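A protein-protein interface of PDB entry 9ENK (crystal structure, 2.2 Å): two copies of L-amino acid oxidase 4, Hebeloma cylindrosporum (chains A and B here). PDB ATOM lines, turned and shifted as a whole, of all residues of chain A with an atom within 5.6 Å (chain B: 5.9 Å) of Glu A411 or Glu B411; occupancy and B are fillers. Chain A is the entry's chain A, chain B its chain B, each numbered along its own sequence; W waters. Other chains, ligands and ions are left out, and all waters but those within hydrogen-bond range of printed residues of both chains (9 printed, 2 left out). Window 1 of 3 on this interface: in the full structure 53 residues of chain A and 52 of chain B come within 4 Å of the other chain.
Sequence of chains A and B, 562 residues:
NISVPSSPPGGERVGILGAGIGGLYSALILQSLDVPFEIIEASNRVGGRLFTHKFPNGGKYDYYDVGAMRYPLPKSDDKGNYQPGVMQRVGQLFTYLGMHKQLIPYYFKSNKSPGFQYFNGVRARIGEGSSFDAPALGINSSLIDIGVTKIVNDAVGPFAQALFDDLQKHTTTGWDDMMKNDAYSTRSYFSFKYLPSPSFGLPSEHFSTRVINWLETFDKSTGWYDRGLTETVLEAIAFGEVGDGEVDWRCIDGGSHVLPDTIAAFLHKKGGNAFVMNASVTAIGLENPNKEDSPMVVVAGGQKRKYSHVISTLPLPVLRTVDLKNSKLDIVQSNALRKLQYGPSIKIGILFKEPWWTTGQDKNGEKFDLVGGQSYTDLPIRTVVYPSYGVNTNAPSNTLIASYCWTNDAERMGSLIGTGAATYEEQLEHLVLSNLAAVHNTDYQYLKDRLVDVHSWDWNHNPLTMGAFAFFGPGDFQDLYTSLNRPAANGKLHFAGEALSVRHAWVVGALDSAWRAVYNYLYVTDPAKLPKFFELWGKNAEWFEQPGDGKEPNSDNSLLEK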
ATOM      1  N   ARG A 227     -20.729  -5.058 -20.416  1.00  0.00           N
ATOM      2  CA  ARG A 227     -19.492  -4.956 -19.674  1.00  0.00           C
ATOM      3  C   ARG A 227     -18.364  -4.594 -20.639  1.00  0.00           C
ATOM      4  O   ARG A 227     -18.571  -4.409 -21.845  1.00  0.00           O
ATOM      5  CB  ARG A 227     -19.211  -6.260 -18.941  1.00  0.00           C
ATOM      6  CG  ARG A 227     -20.419  -6.782 -18.193  1.00  0.00           C
ATOM      7  CD  ARG A 227     -20.256  -6.641 -16.726  1.00  0.00           C
ATOM      8  NE  ARG A 227     -21.489  -6.934 -16.000  1.00  0.00           N
ATOM      9  CZ  ARG A 227     -21.567  -6.954 -14.677  1.00  0.00           C
ATOM     10  NH1 ARG A 227     -20.494  -6.752 -13.924  1.00  0.00           N
ATOM     11  NH2 ARG A 227     -22.747  -7.159 -14.096  1.00  0.00           N
ATOM     12  N   GLN A 341     -15.768  -3.050 -11.277  1.00  0.00           N
ATOM     13  CA  GLN A 341     -17.066  -3.708 -11.213  1.00  0.00           C
ATOM     14  C   GLN A 341     -16.946  -5.207 -11.001  1.00  0.00           C
ATOM     15  O   GLN A 341     -16.079  -5.866 -11.574  1.00  0.00           O
ATOM     16  CB  GLN A 341     -17.866  -3.440 -12.499  1.00  0.00           C
ATOM     17  CG  GLN A 341     -19.318  -3.848 -12.395  1.00  0.00           C
ATOM     18  CD  GLN A 341     -20.160  -3.437 -13.587  1.00  0.00           C
ATOM     19  OE1 GLN A 341     -21.348  -3.202 -13.447  1.00  0.00           O
ATOM     20  NE2 GLN A 341     -19.547  -3.362 -14.764  1.00  0.00           N
ATOM     21  N   TYR A 342     -17.852  -5.743 -10.195  1.00  0.00           N
ATOM     22  CA  TYR A 342     -18.004  -7.173  -9.989  1.00  0.00           C
ATOM     23  C   TYR A 342     -19.213  -7.682 -10.766  1.00  0.00           C
ATOM     24  O   TYR A 342     -20.106  -6.917 -11.143  1.00  0.00           O
ATOM     25  CB  TYR A 342     -18.157  -7.503  -8.496  1.00  0.00           C
ATOM     26  CG  TYR A 342     -16.815  -7.705  -7.815  1.00  0.00           C
ATOM     27  CD1 TYR A 342     -15.860  -6.694  -7.821  1.00  0.00           C
ATOM     28  CD2 TYR A 342     -16.496  -8.907  -7.203  1.00  0.00           C
ATOM     29  CE1 TYR A 342     -14.629  -6.871  -7.226  1.00  0.00           C
ATOM     30  CE2 TYR A 342     -15.260  -9.093  -6.601  1.00  0.00           C
ATOM     31  CZ  TYR A 342     -14.334  -8.071  -6.620  1.00  0.00           C
ATOM     32  OH  TYR A 342     -13.099  -8.235  -6.043  1.00  0.00           O
ATOM     33  N   PRO A 344     -22.196 -11.021 -11.141  1.00  0.00           N
ATOM     34  CA  PRO A 344     -22.926 -12.008 -10.341  1.00  0.00           C
ATOM     35  C   PRO A 344     -22.870 -13.406 -10.949  1.00  0.00           C
ATOM     36  O   PRO A 344     -22.525 -13.595 -12.121  1.00  0.00           O
ATOM     37  CB  PRO A 344     -24.360 -11.464 -10.379  1.00  0.00           C
ATOM     38  CG  PRO A 344     -24.449 -10.892 -11.794  1.00  0.00           C
ATOM     39  CD  PRO A 344     -23.070 -10.334 -12.109  1.00  0.00           C
ATOM     40  N   ILE A 346     -24.914 -17.557 -10.152  1.00  0.00           N
ATOM     41  CA  ILE A 346     -25.612 -18.526  -9.321  1.00  0.00           C
ATOM     42  C   ILE A 346     -25.384 -19.909  -9.904  1.00  0.00           C
ATOM     43  O   ILE A 346     -25.106 -20.067 -11.099  1.00  0.00           O
ATOM     44  CB  ILE A 346     -27.126 -18.259  -9.202  1.00  0.00           C
ATOM     45  CG1 ILE A 346     -27.828 -18.500 -10.535  1.00  0.00           C
ATOM     46  CG2 ILE A 346     -27.365 -16.838  -8.729  1.00  0.00           C
ATOM     47  CD1 ILE A 346     -28.336 -19.951 -10.737  1.00  0.00           C
ATOM     48  N   TRP A 406     -25.012 -16.231 -15.363  1.00  0.00           N
ATOM     49  CA  TRP A 406     -24.195 -15.039 -15.254  1.00  0.00           C
ATOM     50  C   TRP A 406     -25.059 -13.789 -15.429  1.00  0.00           C
ATOM     51  O   TRP A 406     -26.231 -13.861 -15.814  1.00  0.00           O
ATOM     52  CB  TRP A 406     -23.085 -15.044 -16.312  1.00  0.00           C
ATOM     53  CG  TRP A 406     -22.092 -16.141 -16.183  1.00  0.00           C
ATOM     54  CD1 TRP A 406     -21.710 -16.769 -15.043  1.00  0.00           C
ATOM     55  CD2 TRP A 406     -21.337 -16.737 -17.243  1.00  0.00           C
ATOM     56  NE1 TRP A 406     -20.768 -17.725 -15.319  1.00  0.00           N
ATOM     57  CE2 TRP A 406     -20.514 -17.723 -16.664  1.00  0.00           C
ATOM     58  CE3 TRP A 406     -21.273 -16.530 -18.629  1.00  0.00           C
ATOM     59  CZ2 TRP A 406     -19.631 -18.503 -17.419  1.00  0.00           C
ATOM     60  CZ3 TRP A 406     -20.394 -17.307 -19.384  1.00  0.00           C
ATOM     61  CH2 TRP A 406     -19.587 -18.281 -18.775  1.00  0.00           C
ATOM     62  N   THR A 407     -24.446 -12.625 -15.150  1.00  0.00           N
ATOM     63  CA  THR A 407     -25.036 -11.318 -15.442  1.00  0.00           C
ATOM     64  C   THR A 407     -26.533 -11.269 -15.141  1.00  0.00           C
ATOM     65  O   THR A 407     -26.946 -11.668 -14.046  1.00  0.00           O
ATOM     66  CB  THR A 407     -24.717 -10.920 -16.887  1.00  0.00           C
ATOM     67  OG1 THR A 407     -25.071 -11.960 -17.801  1.00  0.00           O
ATOM     68  CG2 THR A 407     -23.216 -10.656 -17.047  1.00  0.00           C
ATOM     69  N   ASN A 408     -27.352 -10.736 -16.053  1.00  0.00           N
ATOM     70  CA  ASN A 408     -28.762 -10.520 -15.728  1.00  0.00           C
ATOM     71  C   ASN A 408     -29.458 -11.829 -15.343  1.00  0.00           C
ATOM     72  O   ASN A 408     -30.351 -11.844 -14.489  1.00  0.00           O
ATOM     73  CB  ASN A 408     -29.508  -9.879 -16.901  1.00  0.00           C
ATOM     74  CG  ASN A 408     -29.042  -8.474 -17.230  1.00  0.00           C
ATOM     75  OD1 ASN A 408     -29.222  -8.018 -18.359  1.00  0.00           O
ATOM     76  ND2 ASN A 408     -28.456  -7.780 -16.262  1.00  0.00           N
ATOM     77  N   ASP A 409     -29.114 -12.932 -16.013  1.00  0.00           N
ATOM     78  CA  ASP A 409     -29.770 -14.197 -15.714  1.00  0.00           C
ATOM     79  C   ASP A 409     -29.517 -14.595 -14.264  1.00  0.00           C
ATOM     80  O   ASP A 409     -30.423 -15.079 -13.578  1.00  0.00           O
ATOM     81  CB  ASP A 409     -29.275 -15.292 -16.667  1.00  0.00           C
ATOM     82  CG  ASP A 409     -29.375 -14.886 -18.121  1.00  0.00           C
ATOM     83  OD1 ASP A 409     -30.471 -14.434 -18.550  1.00  0.00           O
ATOM     84  OD2 ASP A 409     -28.351 -15.005 -18.837  1.00  0.00           O
ATOM     85  N   ALA A 410     -28.295 -14.372 -13.776  1.00  0.00           N
ATOM     86  CA  ALA A 410     -27.980 -14.699 -12.388  1.00  0.00           C
ATOM     87  C   ALA A 410     -28.640 -13.724 -11.424  1.00  0.00           C
ATOM     88  O   ALA A 410     -29.084 -14.121 -10.345  1.00  0.00           O
ATOM     89  CB  ALA A 410     -26.464 -14.697 -12.178  1.00  0.00           C
ATOM     90  N   GLU A 411     -28.699 -12.441 -11.792  1.00  0.00           N
ATOM     91  CA  GLU A 411     -29.371 -11.455 -10.949  1.00  0.00           C
ATOM     92  C   GLU A 411     -30.843 -11.809 -10.764  1.00  0.00           C
ATOM     93  O   GLU A 411     -31.370 -11.790  -9.641  1.00  0.00           O
ATOM     94  CB  GLU A 411     -29.220 -10.059 -11.561  1.00  0.00           C
ATOM     95  CG  GLU A 411     -27.778  -9.540 -11.489  1.00  0.00           C
ATOM     96  CD  GLU A 411     -27.492  -8.475 -12.515  1.00  0.00           C
ATOM     97  OE1 GLU A 411     -28.411  -8.134 -13.285  1.00  0.00           O
ATOM     98  OE2 GLU A 411     -26.333  -7.998 -12.572  1.00  0.00           O
ATOM     99  N   ARG A 412     -31.529 -12.139 -11.863  1.00  0.00           N
ATOM    100  CA  ARG A 412     -32.937 -12.490 -11.754  1.00  0.00           C
ATOM    101  C   ARG A 412     -33.124 -13.766 -10.945  1.00  0.00           C
ATOM    102  O   ARG A 412     -33.918 -13.802 -10.003  1.00  0.00           O
ATOM    103  CB  ARG A 412     -33.544 -12.632 -13.148  1.00  0.00           C
ATOM    104  CG  ARG A 412     -33.574 -11.337 -13.928  1.00  0.00           C
ATOM    105  CD  ARG A 412     -34.097 -11.545 -15.329  1.00  0.00           C
ATOM    106  NE  ARG A 412     -34.410 -10.272 -15.961  1.00  0.00           N
ATOM    107  CZ  ARG A 412     -35.233 -10.125 -16.983  1.00  0.00           C
ATOM    108  NH1 ARG A 412     -35.849 -11.158 -17.527  1.00  0.00           N
ATOM    109  NH2 ARG A 412     -35.447  -8.909 -17.466  1.00  0.00           N
ATOM    110  N   MET A 413     -32.390 -14.824 -11.283  1.00  0.00           N
ATOM    111  CA  MET A 413     -32.579 -16.087 -10.570  1.00  0.00           C
ATOM    112  C   MET A 413     -32.248 -15.954  -9.087  1.00  0.00           C
ATOM    113  O   MET A 413     -32.817 -16.674  -8.259  1.00  0.00           O
ATOM    114  CB  MET A 413     -31.725 -17.183 -11.197  1.00  0.00           C
ATOM    115  CG  MET A 413     -32.074 -18.590 -10.692  1.00  0.00           C
ATOM    116  SD  MET A 413     -33.628 -19.214 -11.358  1.00  0.00           S
ATOM    117  CE  MET A 413     -33.147 -19.774 -12.987  1.00  0.00           C
ATOM    118  N   GLY A 414     -31.337 -15.041  -8.734  1.00  0.00           N
ATOM    119  CA  GLY A 414     -30.938 -14.904  -7.343  1.00  0.00           C
ATOM    120  C   GLY A 414     -32.080 -14.580  -6.405  1.00  0.00           C
ATOM    121  O   GLY A 414     -32.030 -14.925  -5.216  1.00  0.00           O
ATOM    122  N   SER A 415     -33.136 -13.940  -6.917  1.00  0.00           N
ATOM    123  CA  SER A 415     -34.267 -13.598  -6.067  1.00  0.00           C
ATOM    124  C   SER A 415     -35.006 -14.826  -5.555  1.00  0.00           C
ATOM    125  O   SER A 415     -35.750 -14.717  -4.574  1.00  0.00           O
ATOM    126  CB  SER A 415     -35.246 -12.688  -6.804  1.00  0.00           C
ATOM    127  OG  SER A 415     -34.916 -11.330  -6.618  1.00  0.00           O
ATOM    128  N   ASN A 460     -23.783 -13.559  -5.423  1.00  0.00           N
ATOM    129  CA  ASN A 460     -24.092 -12.147  -5.258  1.00  0.00           C
ATOM    130  C   ASN A 460     -24.972 -11.885  -4.044  1.00  0.00           C
ATOM    131  O   ASN A 460     -25.433 -10.747  -3.854  1.00  0.00           O
ATOM    132  CB  ASN A 460     -24.758 -11.598  -6.511  1.00  0.00           C
ATOM    133  CG  ASN A 460     -24.606 -10.116  -6.625  1.00  0.00           C
ATOM    134  OD1 ASN A 460     -23.601  -9.555  -6.182  1.00  0.00           O
ATOM    135  ND2 ASN A 460     -25.609  -9.455  -7.196  1.00  0.00           N
ATOM    136  N   MET A 466     -19.577 -10.952  -1.899  1.00  0.00           N
ATOM    137  CA  MET A 466     -20.275  -9.740  -2.336  1.00  0.00           C
ATOM    138  C   MET A 466     -20.218  -9.601  -3.852  1.00  0.00           C
ATOM    139  O   MET A 466     -19.940  -8.537  -4.406  1.00  0.00           O
ATOM    140  CB  MET A 466     -19.703  -8.512  -1.629  1.00  0.00           C
ATOM    141  CG  MET A 466     -19.790  -8.616  -0.112  1.00  0.00           C
ATOM    142  SD  MET A 466     -19.139  -7.183   0.769  1.00  0.00           S
ATOM    143  CE  MET A 466     -20.470  -6.002   0.511  1.00  0.00           C
ATOM    144  N   ARG B 227     -25.467   1.829 -18.205  1.00  0.00           N
ATOM    145  CA  ARG B 227     -26.806   1.578 -18.703  1.00  0.00           C
ATOM    146  C   ARG B 227     -27.083   2.512 -19.877  1.00  0.00           C
ATOM    147  O   ARG B 227     -26.244   3.339 -20.265  1.00  0.00           O
ATOM    148  CB  ARG B 227     -27.830   1.761 -17.590  1.00  0.00           C
ATOM    149  CG  ARG B 227     -27.456   1.042 -16.319  1.00  0.00           C
ATOM    150  CD  ARG B 227     -28.324  -0.138 -16.099  1.00  0.00           C
ATOM    151  NE  ARG B 227     -27.840  -0.978 -15.014  1.00  0.00           N
ATOM    152  CZ  ARG B 227     -28.482  -2.049 -14.568  1.00  0.00           C
ATOM    153  NH1 ARG B 227     -29.654  -2.402 -15.069  1.00  0.00           N
ATOM    154  NH2 ARG B 227     -27.928  -2.783 -13.610  1.00  0.00           N
ATOM    155  N   GLN B 341     -33.544  -4.887 -19.562  1.00  0.00           N
ATOM    156  CA  GLN B 341     -32.788  -4.998 -18.325  1.00  0.00           C
ATOM    157  C   GLN B 341     -33.489  -4.330 -17.152  1.00  0.00           C
ATOM    158  O   GLN B 341     -34.114  -3.274 -17.286  1.00  0.00           O
ATOM    159  CB  GLN B 341     -31.395  -4.395 -18.498  1.00  0.00           C
ATOM    160  CG  GLN B 341     -30.453  -4.709 -17.364  1.00  0.00           C
ATOM    161  CD  GLN B 341     -29.026  -4.251 -17.647  1.00  0.00           C
ATOM    162  OE1 GLN B 341     -28.068  -4.851 -17.165  1.00  0.00           O
ATOM    163  NE2 GLN B 341     -28.886  -3.183 -18.419  1.00  0.00           N
ATOM    164  N   TYR B 342     -33.374  -4.966 -15.997  1.00  0.00           N
ATOM    165  CA  TYR B 342     -33.807  -4.434 -14.716  1.00  0.00           C
ATOM    166  C   TYR B 342     -32.598  -3.954 -13.907  1.00  0.00           C
ATOM    167  O   TYR B 342     -31.456  -4.369 -14.133  1.00  0.00           O
ATOM    168  CB  TYR B 342     -34.583  -5.500 -13.931  1.00  0.00           C
ATOM    169  CG  TYR B 342     -36.062  -5.516 -14.252  1.00  0.00           C
ATOM    170  CD1 TYR B 342     -36.510  -5.712 -15.550  1.00  0.00           C
ATOM    171  CD2 TYR B 342     -37.010  -5.318 -13.252  1.00  0.00           C
ATOM    172  CE1 TYR B 342     -37.858  -5.708 -15.855  1.00  0.00           C
ATOM    173  CE2 TYR B 342     -38.373  -5.308 -13.551  1.00  0.00           C
ATOM    174  CZ  TYR B 342     -38.784  -5.508 -14.856  1.00  0.00           C
ATOM    175  OH  TYR B 342     -40.130  -5.513 -15.166  1.00  0.00           O
ATOM    176  N   PRO B 344     -31.123  -2.923  -9.793  1.00  0.00           N
ATOM    177  CA  PRO B 344     -31.302  -3.263  -8.382  1.00  0.00           C
ATOM    178  C   PRO B 344     -31.421  -2.015  -7.519  1.00  0.00           C
ATOM    179  O   PRO B 344     -31.084  -0.904  -7.931  1.00  0.00           O
ATOM    180  CB  PRO B 344     -30.016  -4.025  -8.052  1.00  0.00           C
ATOM    181  CG  PRO B 344     -28.981  -3.282  -8.882  1.00  0.00           C
ATOM    182  CD  PRO B 344     -29.695  -2.850 -10.163  1.00  0.00           C
ATOM    183  N   ILE B 346     -31.573  -1.086  -2.919  1.00  0.00           N
ATOM    184  CA  ILE B 346     -31.766  -1.450  -1.525  1.00  0.00           C
ATOM    185  C   ILE B 346     -32.065  -0.191  -0.727  1.00  0.00           C
ATOM    186  O   ILE B 346     -31.681   0.918  -1.106  1.00  0.00           O
ATOM    187  CB  ILE B 346     -30.536  -2.182  -0.931  1.00  0.00           C
ATOM    188  CG1 ILE B 346     -29.334  -1.237  -0.826  1.00  0.00           C
ATOM    189  CG2 ILE B 346     -30.160  -3.386  -1.780  1.00  0.00           C
ATOM    190  CD1 ILE B 346     -29.234  -0.492   0.505  1.00  0.00           C
ATOM    191  N   TRP B 406     -28.336   2.306  -5.624  1.00  0.00           N
ATOM    192  CA  TRP B 406     -28.665   1.835  -6.957  1.00  0.00           C
ATOM    193  C   TRP B 406     -27.487   1.048  -7.525  1.00  0.00           C
ATOM    194  O   TRP B 406     -26.384   1.048  -6.976  1.00  0.00           O
ATOM    195  CB  TRP B 406     -29.007   3.018  -7.879  1.00  0.00           C
ATOM    196  CG  TRP B 406     -30.210   3.801  -7.464  1.00  0.00           C
ATOM    197  CD1 TRP B 406     -31.296   3.339  -6.792  1.00  0.00           C
ATOM    198  CD2 TRP B 406     -30.446   5.194  -7.694  1.00  0.00           C
ATOM    199  NE1 TRP B 406     -32.199   4.349  -6.588  1.00  0.00           N
ATOM    200  CE2 TRP B 406     -31.700   5.502  -7.132  1.00  0.00           C
ATOM    201  CE3 TRP B 406     -29.719   6.213  -8.333  1.00  0.00           C
ATOM    202  CZ2 TRP B 406     -32.254   6.789  -7.193  1.00  0.00           C
ATOM    203  CZ3 TRP B 406     -30.264   7.493  -8.385  1.00  0.00           C
ATOM    204  CH2 TRP B 406     -31.526   7.766  -7.821  1.00  0.00           C
ATOM    205  N   THR B 407     -27.735   0.386  -8.660  1.00  0.00           N
ATOM    206  CA  THR B 407     -26.696  -0.275  -9.448  1.00  0.00           C
ATOM    207  C   THR B 407     -25.667  -0.997  -8.583  1.00  0.00           C
ATOM    208  O   THR B 407     -26.052  -1.763  -7.698  1.00  0.00           O
ATOM    209  CB  THR B 407     -26.032   0.748 -10.373  1.00  0.00           C
ATOM    210  OG1 THR B 407     -25.549   1.871  -9.617  1.00  0.00           O
ATOM    211  CG2 THR B 407     -27.048   1.256 -11.391  1.00  0.00           C
ATOM    212  N   ASN B 408     -24.372  -0.808  -8.854  1.00  0.00           N
ATOM    213  CA  ASN B 408     -23.352  -1.609  -8.175  1.00  0.00           C
ATOM    214  C   ASN B 408     -23.412  -1.430  -6.657  1.00  0.00           C
ATOM    215  O   ASN B 408     -23.172  -2.376  -5.892  1.00  0.00           O
ATOM    216  CB  ASN B 408     -21.946  -1.250  -8.668  1.00  0.00           C
ATOM    217  CG  ASN B 408     -21.709  -1.568 -10.135  1.00  0.00           C
ATOM    218  OD1 ASN B 408     -20.829  -0.971 -10.757  1.00  0.00           O
ATOM    219  ND2 ASN B 408     -22.478  -2.493 -10.695  1.00  0.00           N
ATOM    220  N   ASP B 409     -23.685  -0.210  -6.197  1.00  0.00           N
ATOM    221  CA  ASP B 409     -23.718   0.026  -4.758  1.00  0.00           C
ATOM    222  C   ASP B 409     -24.787  -0.834  -4.101  1.00  0.00           C
ATOM    223  O   ASP B 409     -24.574  -1.388  -3.015  1.00  0.00           O
ATOM    224  CB  ASP B 409     -23.969   1.504  -4.465  1.00  0.00           C
ATOM    225  CG  ASP B 409     -23.007   2.417  -5.201  1.00  0.00           C
ATOM    226  OD1 ASP B 409     -21.773   2.193  -5.111  1.00  0.00           O
ATOM    227  OD2 ASP B 409     -23.495   3.353  -5.880  1.00  0.00           O
ATOM    228  N   ALA B 410     -25.937  -0.970  -4.759  1.00  0.00           N
ATOM    229  CA  ALA B 410     -27.017  -1.788  -4.230  1.00  0.00           C
ATOM    230  C   ALA B 410     -26.698  -3.268  -4.351  1.00  0.00           C
ATOM    231  O   ALA B 410     -27.016  -4.049  -3.446  1.00  0.00           O
ATOM    232  CB  ALA B 410     -28.321  -1.460  -4.961  1.00  0.00           C
ATOM    233  N   GLU B 411     -26.064  -3.671  -5.458  1.00  0.00           N
ATOM    234  CA  GLU B 411     -25.661  -5.069  -5.613  1.00  0.00           C
ATOM    235  C   GLU B 411     -24.716  -5.497  -4.498  1.00  0.00           C
ATOM    236  O   GLU B 411     -24.902  -6.552  -3.872  1.00  0.00           O
ATOM    237  CB  GLU B 411     -25.007  -5.272  -6.980  1.00  0.00           C
ATOM    238  CG  GLU B 411     -26.004  -5.172  -8.130  1.00  0.00           C
ATOM    239  CD  GLU B 411     -25.349  -4.791  -9.461  1.00  0.00           C
ATOM    240  OE1 GLU B 411     -24.104  -4.606  -9.505  1.00  0.00           O
ATOM    241  OE2 GLU B 411     -26.102  -4.665 -10.453  1.00  0.00           O
ATOM    242  N   ARG B 412     -23.700  -4.678  -4.222  1.00  0.00           N
ATOM    243  CA  ARG B 412     -22.745  -5.024  -3.175  1.00  0.00           C
ATOM    244  C   ARG B 412     -23.419  -5.054  -1.809  1.00  0.00           C
ATOM    245  O   ARG B 412     -23.307  -6.040  -1.078  1.00  0.00           O
ATOM    246  CB  ARG B 412     -21.575  -4.036  -3.193  1.00  0.00           C
ATOM    247  CG  ARG B 412     -20.750  -4.108  -4.477  1.00  0.00           C
ATOM    248  CD  ARG B 412     -19.646  -3.078  -4.483  1.00  0.00           C
ATOM    249  NE  ARG B 412     -18.670  -3.318  -5.542  1.00  0.00           N
ATOM    250  CZ  ARG B 412     -17.429  -2.853  -5.529  1.00  0.00           C
ATOM    251  NH1 ARG B 412     -16.976  -2.125  -4.525  1.00  0.00           N
ATOM    252  NH2 ARG B 412     -16.616  -3.149  -6.535  1.00  0.00           N
ATOM    253  N   MET B 413     -24.150  -3.992  -1.459  1.00  0.00           N
ATOM    254  CA  MET B 413     -24.790  -3.946  -0.144  1.00  0.00           C
ATOM    255  C   MET B 413     -25.809  -5.065   0.028  1.00  0.00           C
ATOM    256  O   MET B 413     -26.070  -5.501   1.157  1.00  0.00           O
ATOM    257  CB  MET B 413     -25.473  -2.602   0.070  1.00  0.00           C
ATOM    258  CG  MET B 413     -25.941  -2.371   1.501  1.00  0.00           C
ATOM    259  SD  MET B 413     -24.598  -2.012   2.651  1.00  0.00           S
ATOM    260  CE  MET B 413     -24.311  -0.277   2.305  1.00  0.00           C
ATOM    261  N   GLY B 414     -26.409  -5.527  -1.070  1.00  0.00           N
ATOM    262  CA  GLY B 414     -27.419  -6.564  -0.974  1.00  0.00           C
ATOM    263  C   GLY B 414     -26.914  -7.839  -0.332  1.00  0.00           C
ATOM    264  O   GLY B 414     -27.700  -8.596   0.254  1.00  0.00           O
ATOM    265  N   SER B 415     -25.606  -8.102  -0.430  1.00  0.00           N
ATOM    266  CA  SER B 415     -25.068  -9.319   0.157  1.00  0.00           C
ATOM    267  C   SER B 415     -25.158  -9.314   1.677  1.00  0.00           C
ATOM    268  O   SER B 415     -25.122 -10.385   2.289  1.00  0.00           O
ATOM    269  CB  SER B 415     -23.611  -9.524  -0.267  1.00  0.00           C
ATOM    270  OG  SER B 415     -23.523 -10.219  -1.494  1.00  0.00           O
ATOM    271  N   ASP B 458     -33.893  -5.564   0.096  1.00  0.00           N
ATOM    272  CA  ASP B 458     -33.162  -5.717  -1.158  1.00  0.00           C
ATOM    273  C   ASP B 458     -34.177  -6.099  -2.230  1.00  0.00           C
ATOM    274  O   ASP B 458     -34.594  -7.256  -2.315  1.00  0.00           O
ATOM    275  CB  ASP B 458     -32.069  -6.769  -1.026  1.00  0.00           C
ATOM    276  CG  ASP B 458     -31.263  -6.953  -2.294  1.00  0.00           C
ATOM    277  OD1 ASP B 458     -31.579  -6.315  -3.308  1.00  0.00           O
ATOM    278  OD2 ASP B 458     -30.280  -7.745  -2.258  1.00  0.00           O
ATOM    279  N   ASN B 460     -33.637  -6.584  -5.163  1.00  0.00           N
ATOM    280  CA  ASN B 460     -33.032  -7.561  -6.057  1.00  0.00           C
ATOM    281  C   ASN B 460     -32.891  -8.930  -5.404  1.00  0.00           C
ATOM    282  O   ASN B 460     -32.223  -9.812  -5.955  1.00  0.00           O
ATOM    283  CB  ASN B 460     -31.675  -7.072  -6.546  1.00  0.00           C
ATOM    284  CG  ASN B 460     -31.285  -7.704  -7.858  1.00  0.00           C
ATOM    285  OD1 ASN B 460     -32.142  -8.002  -8.698  1.00  0.00           O
ATOM    286  ND2 ASN B 460     -29.989  -7.929  -8.043  1.00  0.00           N
ATOM    287  N   MET B 466     -37.905  -9.390  -8.393  1.00  0.00           N
ATOM    288  CA  MET B 466     -36.747  -9.905  -9.124  1.00  0.00           C
ATOM    289  C   MET B 466     -35.963  -8.750  -9.742  1.00  0.00           C
ATOM    290  O   MET B 466     -35.563  -8.772 -10.910  1.00  0.00           O
ATOM    291  CB  MET B 466     -37.185 -10.920 -10.181  1.00  0.00           C
ATOM    292  CG  MET B 466     -37.999 -12.065  -9.595  1.00  0.00           C
ATOM    293  SD  MET B 466     -38.495 -13.329 -10.780  1.00  0.00           S
ATOM    294  CE  MET B 466     -36.989 -14.249 -10.967  1.00  0.00           C
HETATM  295  O   HOH W   1     -19.270  -3.997  -8.378  1.00  0.00           O
HETATM  296  O   HOH W   2     -32.683  -7.813 -15.979  1.00  0.00           O
HETATM  297  O   HOH W   3     -22.735  -6.266 -11.297  1.00  0.00           O
HETATM  298  O   HOH W   4     -29.001  -5.343 -13.390  1.00  0.00           O
HETATM  299  O   HOH W   5     -30.484 -11.537  -7.218  1.00  0.00           O
HETATM  300  O   HOH W   6     -24.912  -7.906 -10.167  1.00  0.00           O
HETATM  301  O   HOH W   7     -25.748  -5.343 -12.974  1.00  0.00           O
HETATM  302  O   HOH W   8     -28.433  -6.336 -10.509  1.00  0.00           O
HETATM  303  O   HOH W   9     -26.924  -8.271  -3.669  1.00  0.00           O
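Of the 18 printed residues of chain B, 8 touch a printed residue of chain A.
Hydrophobic or aromatic side chains of chain B within 4 Å of the printed part of chain A: Tyr B342 and Met B466.
Along chain A the printed residues that touch a printed residue of chain B span positions 341 to 466.
Among the printed residues, no Asp or Glu carboxylate lies within 4 Å of a Lys or Arg side-chain nitrogen of the other chain.
The side-chain amide nitrogen (ND2) of Asn B408 is in hydrogen-bond range of the side-chain amide oxygen (OE1) of Gln A341.
OE1 of Gln B341 lies within hydrogen-bond range of ND2 of Asn A408, 3.1 Å away.
OG of Ser A415 lies within hydrogen-bond range of O of Asn B460.
The side-chain hydroxyl (OG) of Ser B415 is in hydrogen-bond range of the backbone carbonyl oxygen (O) of Asn A460, at 3.1 Å.
The side-chain carboxylate (OE1) of Glu A411 is in hydrogen-bond range of the side-chain amide nitrogen (ND2) of Asn A408 (3.0 Å).
The guanidinium group (NH1) of Arg B227 is in hydrogen-bond range of the backbone carbonyl oxygen (O) of Tyr B342, 2.8 Å away.
ND2 of Asn B408 sits at hydrogen-bond distance from OE1 of Glu B411, 2.9 Å away.
Gln A341 touches Asn B408, and with the chains exchanged Asn A408 touches Gln B341.
Glu A411 touches Asn B460, but with the chains exchanged Asn A460 does not touch Glu B411 (4.01 Å).
Arg A412 touches Met B466, and with the chains exchanged Met A466 touches Arg B412.
Water W7 lies within hydrogen-bond range of OE2 of Glu B411, OE2 of Glu A411 and NH2 of Arg B227.
Water W6 lies within hydrogen-bond range of OE2 of Glu A411 (2.8 Å), ND2 of Asn A460 (3.4 Å) and OE1 of Glu B411 (3.5 Å).
Water W2 lies within hydrogen-bond range of N of Tyr B342 and NE of Arg A412.
Printed residues of chain B within 4 Å of Asn A408: Gln B341.
Ala B410 touches none of the printed residues of chain A.
Printed residues of chain A within 4 Å of Glu B411: Glu A411 (3.96 Å).
Printed residues of chain A within 4 Å of Arg B412: Tyr A342 (3.8 Å) and Met A466 (3.3 Å).
The nearest residue of chain B that does not touch Glu A411 is Tyr B342 (4.9 Å).
Among the printed residues, merely in contact across the chains: Arg A412 with Met B466 (3.2 Å), Met A466 with Arg B412 (3.3 Å), Met A466 with Ser B415 (3.4 Å), Ser A415 with Met B466 (3.4 Å), Tyr A342 with Arg B412 (3.8 Å), Arg A412 with Tyr B342 (3.9 Å), Glu A411 with Glu B411 (3.96 Å) and Glu A411 with Asn B460 (3.98 Å).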
